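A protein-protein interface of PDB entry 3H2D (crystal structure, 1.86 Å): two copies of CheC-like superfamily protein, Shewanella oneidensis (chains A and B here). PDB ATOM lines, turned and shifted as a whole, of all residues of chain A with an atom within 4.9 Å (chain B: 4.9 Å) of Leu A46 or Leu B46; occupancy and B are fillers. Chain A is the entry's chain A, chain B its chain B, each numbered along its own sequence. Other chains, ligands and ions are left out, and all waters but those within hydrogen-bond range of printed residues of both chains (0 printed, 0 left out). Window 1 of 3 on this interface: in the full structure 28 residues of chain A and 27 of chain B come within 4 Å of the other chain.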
ATOM      1  N   SER A  44     -22.811 -26.040  21.427  1.00  0.00           N
ATOM      2  CA  SER A  44     -21.870 -26.398  22.503  1.00  0.00           C
ATOM      3  C   SER A  44     -21.908 -25.419  23.692  1.00  0.00           C
ATOM      4  O   SER A  44     -22.055 -24.219  23.521  1.00  0.00           O
ATOM      5  CB  SER A  44     -20.436 -26.400  21.959  1.00  0.00           C
ATOM      6  OG  SER A  44     -20.210 -27.366  20.937  1.00  0.00           O
ATOM      7  N   GLY A  45     -21.712 -25.943  24.894  1.00  0.00           N
ATOM      8  CA  GLY A  45     -21.512 -25.110  26.100  1.00  0.00           C
ATOM      9  C   GLY A  45     -20.029 -25.148  26.454  1.00  0.00           C
ATOM     10  O   GLY A  45     -19.441 -26.237  26.464  1.00  0.00           O
ATOM     11  N   LEU A  46     -19.452 -23.973  26.752  1.00  0.00           N
ATOM     12  CA  LEU A  46     -18.040 -23.828  27.009  1.00  0.00           C
ATOM     13  C   LEU A  46     -17.873 -22.993  28.297  1.00  0.00           C
ATOM     14  O   LEU A  46     -18.622 -22.023  28.517  1.00  0.00           O
ATOM     15  CB  LEU A  46     -17.358 -23.109  25.830  1.00  0.00           C
ATOM     16  CG  LEU A  46     -17.220 -23.820  24.472  1.00  0.00           C
ATOM     17  CD1 LEU A  46     -18.538 -23.715  23.728  1.00  0.00           C
ATOM     18  CD2 LEU A  46     -16.141 -23.196  23.608  1.00  0.00           C
ATOM     19  N   ILE A  47     -16.900 -23.349  29.125  1.00  0.00           N
ATOM     20  CA  ILE A  47     -16.674 -22.638  30.381  1.00  0.00           C
ATOM     21  C   ILE A  47     -15.194 -22.752  30.784  1.00  0.00           C
ATOM     22  O   ILE A  47     -14.588 -23.808  30.663  1.00  0.00           O
ATOM     23  CB  ILE A  47     -17.664 -23.151  31.482  1.00  0.00           C
ATOM     24  CG1 ILE A  47     -17.682 -22.255  32.723  1.00  0.00           C
ATOM     25  CG2 ILE A  47     -17.427 -24.635  31.822  1.00  0.00           C
ATOM     26  CD1 ILE A  47     -18.903 -22.532  33.601  1.00  0.00           C
ATOM     27  N   GLY A  48     -14.646 -21.665  31.312  1.00  0.00           N
ATOM     28  CA  GLY A  48     -13.293 -21.646  31.834  1.00  0.00           C
ATOM     29  C   GLY A  48     -13.316 -21.874  33.333  1.00  0.00           C
ATOM     30  O   GLY A  48     -14.337 -21.658  33.985  1.00  0.00           O
ATOM     31  N   LEU A  58     -13.535 -26.394  29.747  1.00  0.00           N
ATOM     32  CA  LEU A  58     -14.463 -27.503  29.487  1.00  0.00           C
ATOM     33  C   LEU A  58     -15.467 -27.096  28.424  1.00  0.00           C
ATOM     34  O   LEU A  58     -15.888 -25.941  28.369  1.00  0.00           O
ATOM     35  CB  LEU A  58     -15.176 -27.874  30.801  1.00  0.00           C
ATOM     36  CG  LEU A  58     -16.233 -28.982  30.705  1.00  0.00           C
ATOM     37  CD1 LEU A  58     -16.276 -29.726  32.059  1.00  0.00           C
ATOM     38  CD2 LEU A  58     -17.632 -28.389  30.348  1.00  0.00           C
ATOM     39  N   SER A  59     -15.812 -28.047  27.555  1.00  0.00           N
ATOM     40  CA  SER A  59     -16.863 -27.880  26.589  1.00  0.00           C
ATOM     41  C   SER A  59     -17.666 -29.176  26.484  1.00  0.00           C
ATOM     42  O   SER A  59     -17.133 -30.288  26.662  1.00  0.00           O
ATOM     43  CB  SER A  59     -16.300 -27.469  25.219  1.00  0.00           C
ATOM     44  OG  SER A  59     -15.475 -28.474  24.670  1.00  0.00           O
ATOM     45  N   THR A  94     -24.334 -27.087  31.232  1.00  0.00           N
ATOM     46  CA  THR A  94     -22.913 -26.801  31.413  1.00  0.00           C
ATOM     47  C   THR A  94     -22.630 -26.374  32.872  1.00  0.00           C
ATOM     48  O   THR A  94     -21.685 -26.878  33.499  1.00  0.00           O
ATOM     49  CB  THR A  94     -22.364 -25.764  30.392  1.00  0.00           C
ATOM     50  OG1 THR A  94     -22.663 -26.199  29.038  1.00  0.00           O
ATOM     51  CG2 THR A  94     -20.837 -25.645  30.565  1.00  0.00           C
ATOM     52  N   THR A 116     -18.237 -18.002  33.647  1.00  0.00           N
ATOM     53  CA  THR A 116     -19.629 -18.166  33.243  1.00  0.00           C
ATOM     54  C   THR A 116     -19.678 -18.811  31.825  1.00  0.00           C
ATOM     55  O   THR A 116     -18.748 -18.649  31.043  1.00  0.00           O
ATOM     56  CB  THR A 116     -20.351 -16.822  33.276  1.00  0.00           C
ATOM     57  OG1 THR A 116     -19.619 -15.902  32.492  1.00  0.00           O
ATOM     58  CG2 THR A 116     -20.438 -16.269  34.751  1.00  0.00           C
ATOM     59  N   PRO A 117     -20.724 -19.560  31.537  1.00  0.00           N
ATOM     60  CA  PRO A 117     -20.801 -20.289  30.284  1.00  0.00           C
ATOM     61  C   PRO A 117     -21.082 -19.429  29.067  1.00  0.00           C
ATOM     62  O   PRO A 117     -21.697 -18.375  29.174  1.00  0.00           O
ATOM     63  CB  PRO A 117     -21.946 -21.267  30.490  1.00  0.00           C
ATOM     64  CG  PRO A 117     -22.602 -20.908  31.701  1.00  0.00           C
ATOM     65  CD  PRO A 117     -21.879 -19.838  32.416  1.00  0.00           C
ATOM     66  N   MET A 118     -20.594 -19.910  27.938  1.00  0.00           N
ATOM     67  CA  MET A 118     -20.898 -19.365  26.634  1.00  0.00           C
ATOM     68  C   MET A 118     -21.415 -20.533  25.820  1.00  0.00           C
ATOM     69  O   MET A 118     -20.976 -21.653  26.009  1.00  0.00           O
ATOM     70  CB  MET A 118     -19.639 -18.815  25.971  1.00  0.00           C
ATOM     71  CG  MET A 118     -19.187 -17.555  26.599  1.00  0.00           C
ATOM     72  SD  MET A 118     -17.473 -16.841  25.968  1.00  0.00           S
ATOM     73  CE  MET A 118     -16.514 -18.030  27.097  1.00  0.00           C
ATOM     74  N   VAL A 120     -22.138 -21.816  21.879  1.00  0.00           N
ATOM     75  CA  VAL A 120     -21.920 -21.719  20.415  1.00  0.00           C
ATOM     76  C   VAL A 120     -23.081 -22.407  19.696  1.00  0.00           C
ATOM     77  O   VAL A 120     -23.414 -23.520  20.037  1.00  0.00           O
ATOM     78  CB  VAL A 120     -20.663 -22.450  19.995  1.00  0.00           C
ATOM     79  CG1 VAL A 120     -20.447 -22.385  18.445  1.00  0.00           C
ATOM     80  CG2 VAL A 120     -19.478 -21.898  20.751  1.00  0.00           C
ATOM     81  N   ILE A 127     -14.475 -27.481  18.507  1.00  0.00           N
ATOM     82  CA  ILE A 127     -13.834 -26.747  19.578  1.00  0.00           C
ATOM     83  C   ILE A 127     -12.418 -27.264  19.769  1.00  0.00           C
ATOM     84  O   ILE A 127     -12.166 -28.485  19.859  1.00  0.00           O
ATOM     85  CB  ILE A 127     -14.627 -26.855  20.941  1.00  0.00           C
ATOM     86  CG1 ILE A 127     -16.189 -26.660  20.807  1.00  0.00           C
ATOM     87  CG2 ILE A 127     -13.985 -25.947  22.021  1.00  0.00           C
ATOM     88  CD1 ILE A 127     -16.671 -25.365  20.289  1.00  0.00           C
ATOM     89  N   SER B  44     -13.687 -18.274  16.381  1.00  0.00           N
ATOM     90  CA  SER B  44     -13.824 -17.416  17.568  1.00  0.00           C
ATOM     91  C   SER B  44     -12.913 -17.912  18.669  1.00  0.00           C
ATOM     92  O   SER B  44     -12.786 -19.123  18.836  1.00  0.00           O
ATOM     93  CB  SER B  44     -15.272 -17.414  18.080  1.00  0.00           C
ATOM     94  OG  SER B  44     -16.152 -16.776  17.183  1.00  0.00           O
ATOM     95  N   GLY B  45     -12.302 -16.973  19.400  1.00  0.00           N
ATOM     96  CA  GLY B  45     -11.552 -17.272  20.622  1.00  0.00           C
ATOM     97  C   GLY B  45     -12.424 -16.914  21.833  1.00  0.00           C
ATOM     98  O   GLY B  45     -12.936 -15.807  21.913  1.00  0.00           O
ATOM     99  N   LEU B  46     -12.592 -17.876  22.744  1.00  0.00           N
ATOM    100  CA  LEU B  46     -13.423 -17.759  23.934  1.00  0.00           C
ATOM    101  C   LEU B  46     -12.583 -18.050  25.183  1.00  0.00           C
ATOM    102  O   LEU B  46     -11.748 -18.959  25.173  1.00  0.00           O
ATOM    103  CB  LEU B  46     -14.578 -18.759  23.902  1.00  0.00           C
ATOM    104  CG  LEU B  46     -15.794 -18.430  23.032  1.00  0.00           C
ATOM    105  CD1 LEU B  46     -15.401 -18.380  21.600  1.00  0.00           C
ATOM    106  CD2 LEU B  46     -16.875 -19.529  23.283  1.00  0.00           C
ATOM    107  N   ILE B  47     -12.812 -17.296  26.252  1.00  0.00           N
ATOM    108  CA  ILE B  47     -12.078 -17.473  27.490  1.00  0.00           C
ATOM    109  C   ILE B  47     -12.900 -16.998  28.663  1.00  0.00           C
ATOM    110  O   ILE B  47     -13.618 -16.004  28.587  1.00  0.00           O
ATOM    111  CB  ILE B  47     -10.697 -16.748  27.434  1.00  0.00           C
ATOM    112  CG1 ILE B  47      -9.727 -17.239  28.529  1.00  0.00           C
ATOM    113  CG2 ILE B  47     -10.859 -15.169  27.354  1.00  0.00           C
ATOM    114  CD1 ILE B  47      -8.254 -16.974  28.203  1.00  0.00           C
ATOM    115  N   GLY B  48     -12.780 -17.722  29.758  1.00  0.00           N
ATOM    116  CA  GLY B  48     -13.394 -17.315  31.027  1.00  0.00           C
ATOM    117  C   GLY B  48     -12.455 -16.502  31.883  1.00  0.00           C
ATOM    118  O   GLY B  48     -11.224 -16.602  31.754  1.00  0.00           O
ATOM    119  N   LEU B  58     -15.332 -13.687  27.795  1.00  0.00           N
ATOM    120  CA  LEU B  58     -14.938 -12.916  26.618  1.00  0.00           C
ATOM    121  C   LEU B  58     -14.957 -13.815  25.384  1.00  0.00           C
ATOM    122  O   LEU B  58     -14.510 -14.945  25.447  1.00  0.00           O
ATOM    123  CB  LEU B  58     -13.514 -12.419  26.790  1.00  0.00           C
ATOM    124  CG  LEU B  58     -12.791 -11.842  25.575  1.00  0.00           C
ATOM    125  CD1 LEU B  58     -13.485 -10.546  25.119  1.00  0.00           C
ATOM    126  CD2 LEU B  58     -11.344 -11.593  25.940  1.00  0.00           C
ATOM    127  N   SER B  59     -15.513 -13.300  24.289  1.00  0.00           N
ATOM    128  CA  SER B  59     -15.422 -13.933  22.953  1.00  0.00           C
ATOM    129  C   SER B  59     -14.921 -12.914  21.933  1.00  0.00           C
ATOM    130  O   SER B  59     -15.307 -11.752  21.958  1.00  0.00           O
ATOM    131  CB  SER B  59     -16.737 -14.578  22.478  1.00  0.00           C
ATOM    132  OG  SER B  59     -17.781 -13.648  22.321  1.00  0.00           O
ATOM    133  N   THR B  94      -6.314 -14.326  21.570  1.00  0.00           N
ATOM    134  CA  THR B  94      -7.227 -14.297  22.718  1.00  0.00           C
ATOM    135  C   THR B  94      -6.477 -14.081  24.045  1.00  0.00           C
ATOM    136  O   THR B  94      -6.909 -13.258  24.913  1.00  0.00           O
ATOM    137  CB  THR B  94      -8.060 -15.594  22.788  1.00  0.00           C
ATOM    138  OG1 THR B  94      -8.803 -15.731  21.584  1.00  0.00           O
ATOM    139  CG2 THR B  94      -9.023 -15.564  23.949  1.00  0.00           C
ATOM    140  N   THR B 116      -8.178 -20.533  30.161  1.00  0.00           N
ATOM    141  CA  THR B 116      -7.399 -20.832  28.990  1.00  0.00           C
ATOM    142  C   THR B 116      -8.295 -20.762  27.720  1.00  0.00           C
ATOM    143  O   THR B 116      -9.474 -21.029  27.782  1.00  0.00           O
ATOM    144  CB  THR B 116      -6.745 -22.184  29.100  1.00  0.00           C
ATOM    145  OG1 THR B 116      -7.746 -23.173  29.332  1.00  0.00           O
ATOM    146  CG2 THR B 116      -5.723 -22.214  30.221  1.00  0.00           C
ATOM    147  N   PRO B 117      -7.702 -20.415  26.563  1.00  0.00           N
ATOM    148  CA  PRO B 117      -8.545 -20.184  25.414  1.00  0.00           C
ATOM    149  C   PRO B 117      -9.161 -21.452  24.840  1.00  0.00           C
ATOM    150  O   PRO B 117      -8.574 -22.510  24.891  1.00  0.00           O
ATOM    151  CB  PRO B 117      -7.586 -19.622  24.365  1.00  0.00           C
ATOM    152  CG  PRO B 117      -6.429 -19.136  25.126  1.00  0.00           C
ATOM    153  CD  PRO B 117      -6.293 -20.132  26.240  1.00  0.00           C
ATOM    154  N   MET B 118     -10.394 -21.325  24.380  1.00  0.00           N
ATOM    155  CA  MET B 118     -10.997 -22.332  23.534  1.00  0.00           C
ATOM    156  C   MET B 118     -11.329 -21.630  22.257  1.00  0.00           C
ATOM    157  O   MET B 118     -11.802 -20.495  22.271  1.00  0.00           O
ATOM    158  CB  MET B 118     -12.263 -22.892  24.148  1.00  0.00           C
ATOM    159  CG  MET B 118     -11.998 -23.889  25.226  1.00  0.00           C
ATOM    160  SD  MET B 118     -13.625 -24.230  26.200  1.00  0.00           S
ATOM    161  CE  MET B 118     -13.614 -22.698  27.394  1.00  0.00           C
ATOM    162  N   VAL B 120     -13.347 -21.881  18.595  1.00  0.00           N
ATOM    163  CA  VAL B 120     -14.453 -22.434  17.870  1.00  0.00           C
ATOM    164  C   VAL B 120     -14.173 -22.234  16.400  1.00  0.00           C
ATOM    165  O   VAL B 120     -13.777 -21.144  15.997  1.00  0.00           O
ATOM    166  CB  VAL B 120     -15.731 -21.670  18.216  1.00  0.00           C
ATOM    167  CG1 VAL B 120     -16.924 -22.184  17.369  1.00  0.00           C
ATOM    168  CG2 VAL B 120     -15.991 -21.726  19.763  1.00  0.00           C
ATOM    169  N   ILE B 127     -22.161 -16.825  19.127  1.00  0.00           N
ATOM    170  CA  ILE B 127     -21.848 -17.073  20.535  1.00  0.00           C
ATOM    171  C   ILE B 127     -22.883 -16.346  21.394  1.00  0.00           C
ATOM    172  O   ILE B 127     -23.212 -15.177  21.141  1.00  0.00           O
ATOM    173  CB  ILE B 127     -20.412 -16.572  20.929  1.00  0.00           C
ATOM    174  CG1 ILE B 127     -19.323 -16.954  19.862  1.00  0.00           C
ATOM    175  CG2 ILE B 127     -20.028 -17.073  22.351  1.00  0.00           C
ATOM    176  CD1 ILE B 127     -19.009 -18.417  19.736  1.00  0.00           C
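O of Leu A58 sits close to SD of Met B118 (3.6 Å).
The backbone carbonyl oxygen (O) of Leu B58 lies close to the side-chain sulfur (SD) of Met A118, at 3.6 Å.
The backbone carbonyl oxygen (O) of Ser A44 lies within hydrogen-bond range of the backbone NH (N) of Val A120 (2.9 Å).
The backbone NH (N) of Leu A46 is in hydrogen-bond range of the backbone carbonyl oxygen (O) of Met A118 (2.9 Å).
N of Ile A47 lies within hydrogen-bond range of O of Leu A58 (2.9 Å).
O of Ser B44 lies within hydrogen-bond range of N of Val B120 (2.8 Å).
N of Leu B46 is in hydrogen-bond range of O of Met B118 (2.8 Å).
The backbone carbonyl oxygen of Ile B47 is in hydrogen-bond range of the backbone NH of Leu B58 (3.0 Å).
Among the printed residues, merely in contact across the chains: Leu A46 with Leu B46 (3.8 Å), Leu A46 with Met B118 (3.8 Å), Ile A47 with Met B118 (3.6 Å), Met A118 with Leu B46 (3.7 Å), Met A118 with Ile B47 (3.8 Å), Val A120 with Val B120 (3.6 Å), Val A120 with Ile B127 (3.7 Å) and Ile A127 with Val B120 (3.7 Å).
Of the printed residues of chain B, Leu A46 touches Leu B46 (3.8 Å) and Met B118 (3.8 Å).
Of the printed residues of chain A, Leu B46 touches Leu A46 and Met A118.
Printed residues of chain B within 4 Å of Ile A127: Val B120 (3.7 Å).
Of the printed residues of chain B, Leu A58 touches Met B118 (3.6 Å).
Thr B116 touches none of the printed residues of chain A.
The nearest printed residue of chain B that does not touch Leu A46 is Val B120 (4.1 Å).
The nearest residue of chain A that does not touch Leu B46 is Val A120 (4.3 Å).
The nearest printed residue of chain A that does not touch Val B120 is Leu A46 (4.1 Å).
Printed residues of chain A that touch a printed residue of chain B: Leu A46, Ile A47, Leu A58, Met A118, Val A120 and Ile A127.
Of the 13 printed residues of chain B, 6 touch a printed residue of chain A.
Along chain B the printed residues that touch a printed residue of chain A span positions 46 to 127.
Among the printed residues, 10 pairs touch across the chains.
Among the printed residues, no Asp or Glu carboxylate lies within 4 Å of a Lys or Arg side-chain nitrogen of the other chain.
Leu A46 touches its own counterpart, Leu B46.
Ile A47 touches Met B118, and with the chains exchanged Met A118 touches Ile B47.
Val B120 touches its own counterpart, Val A120.
Val A120 touches Ile B127, and with the chains exchanged Ile A127 touches Val B120.
Positions printed for both chains: 44, 45, 46, 47, 48, 58, 59, 94, 116, 117, 118, 120 and 127.
Of the 10 pairs that touch across the chains among the printed residues, 10 have their exchanged pair printed and touching as well.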
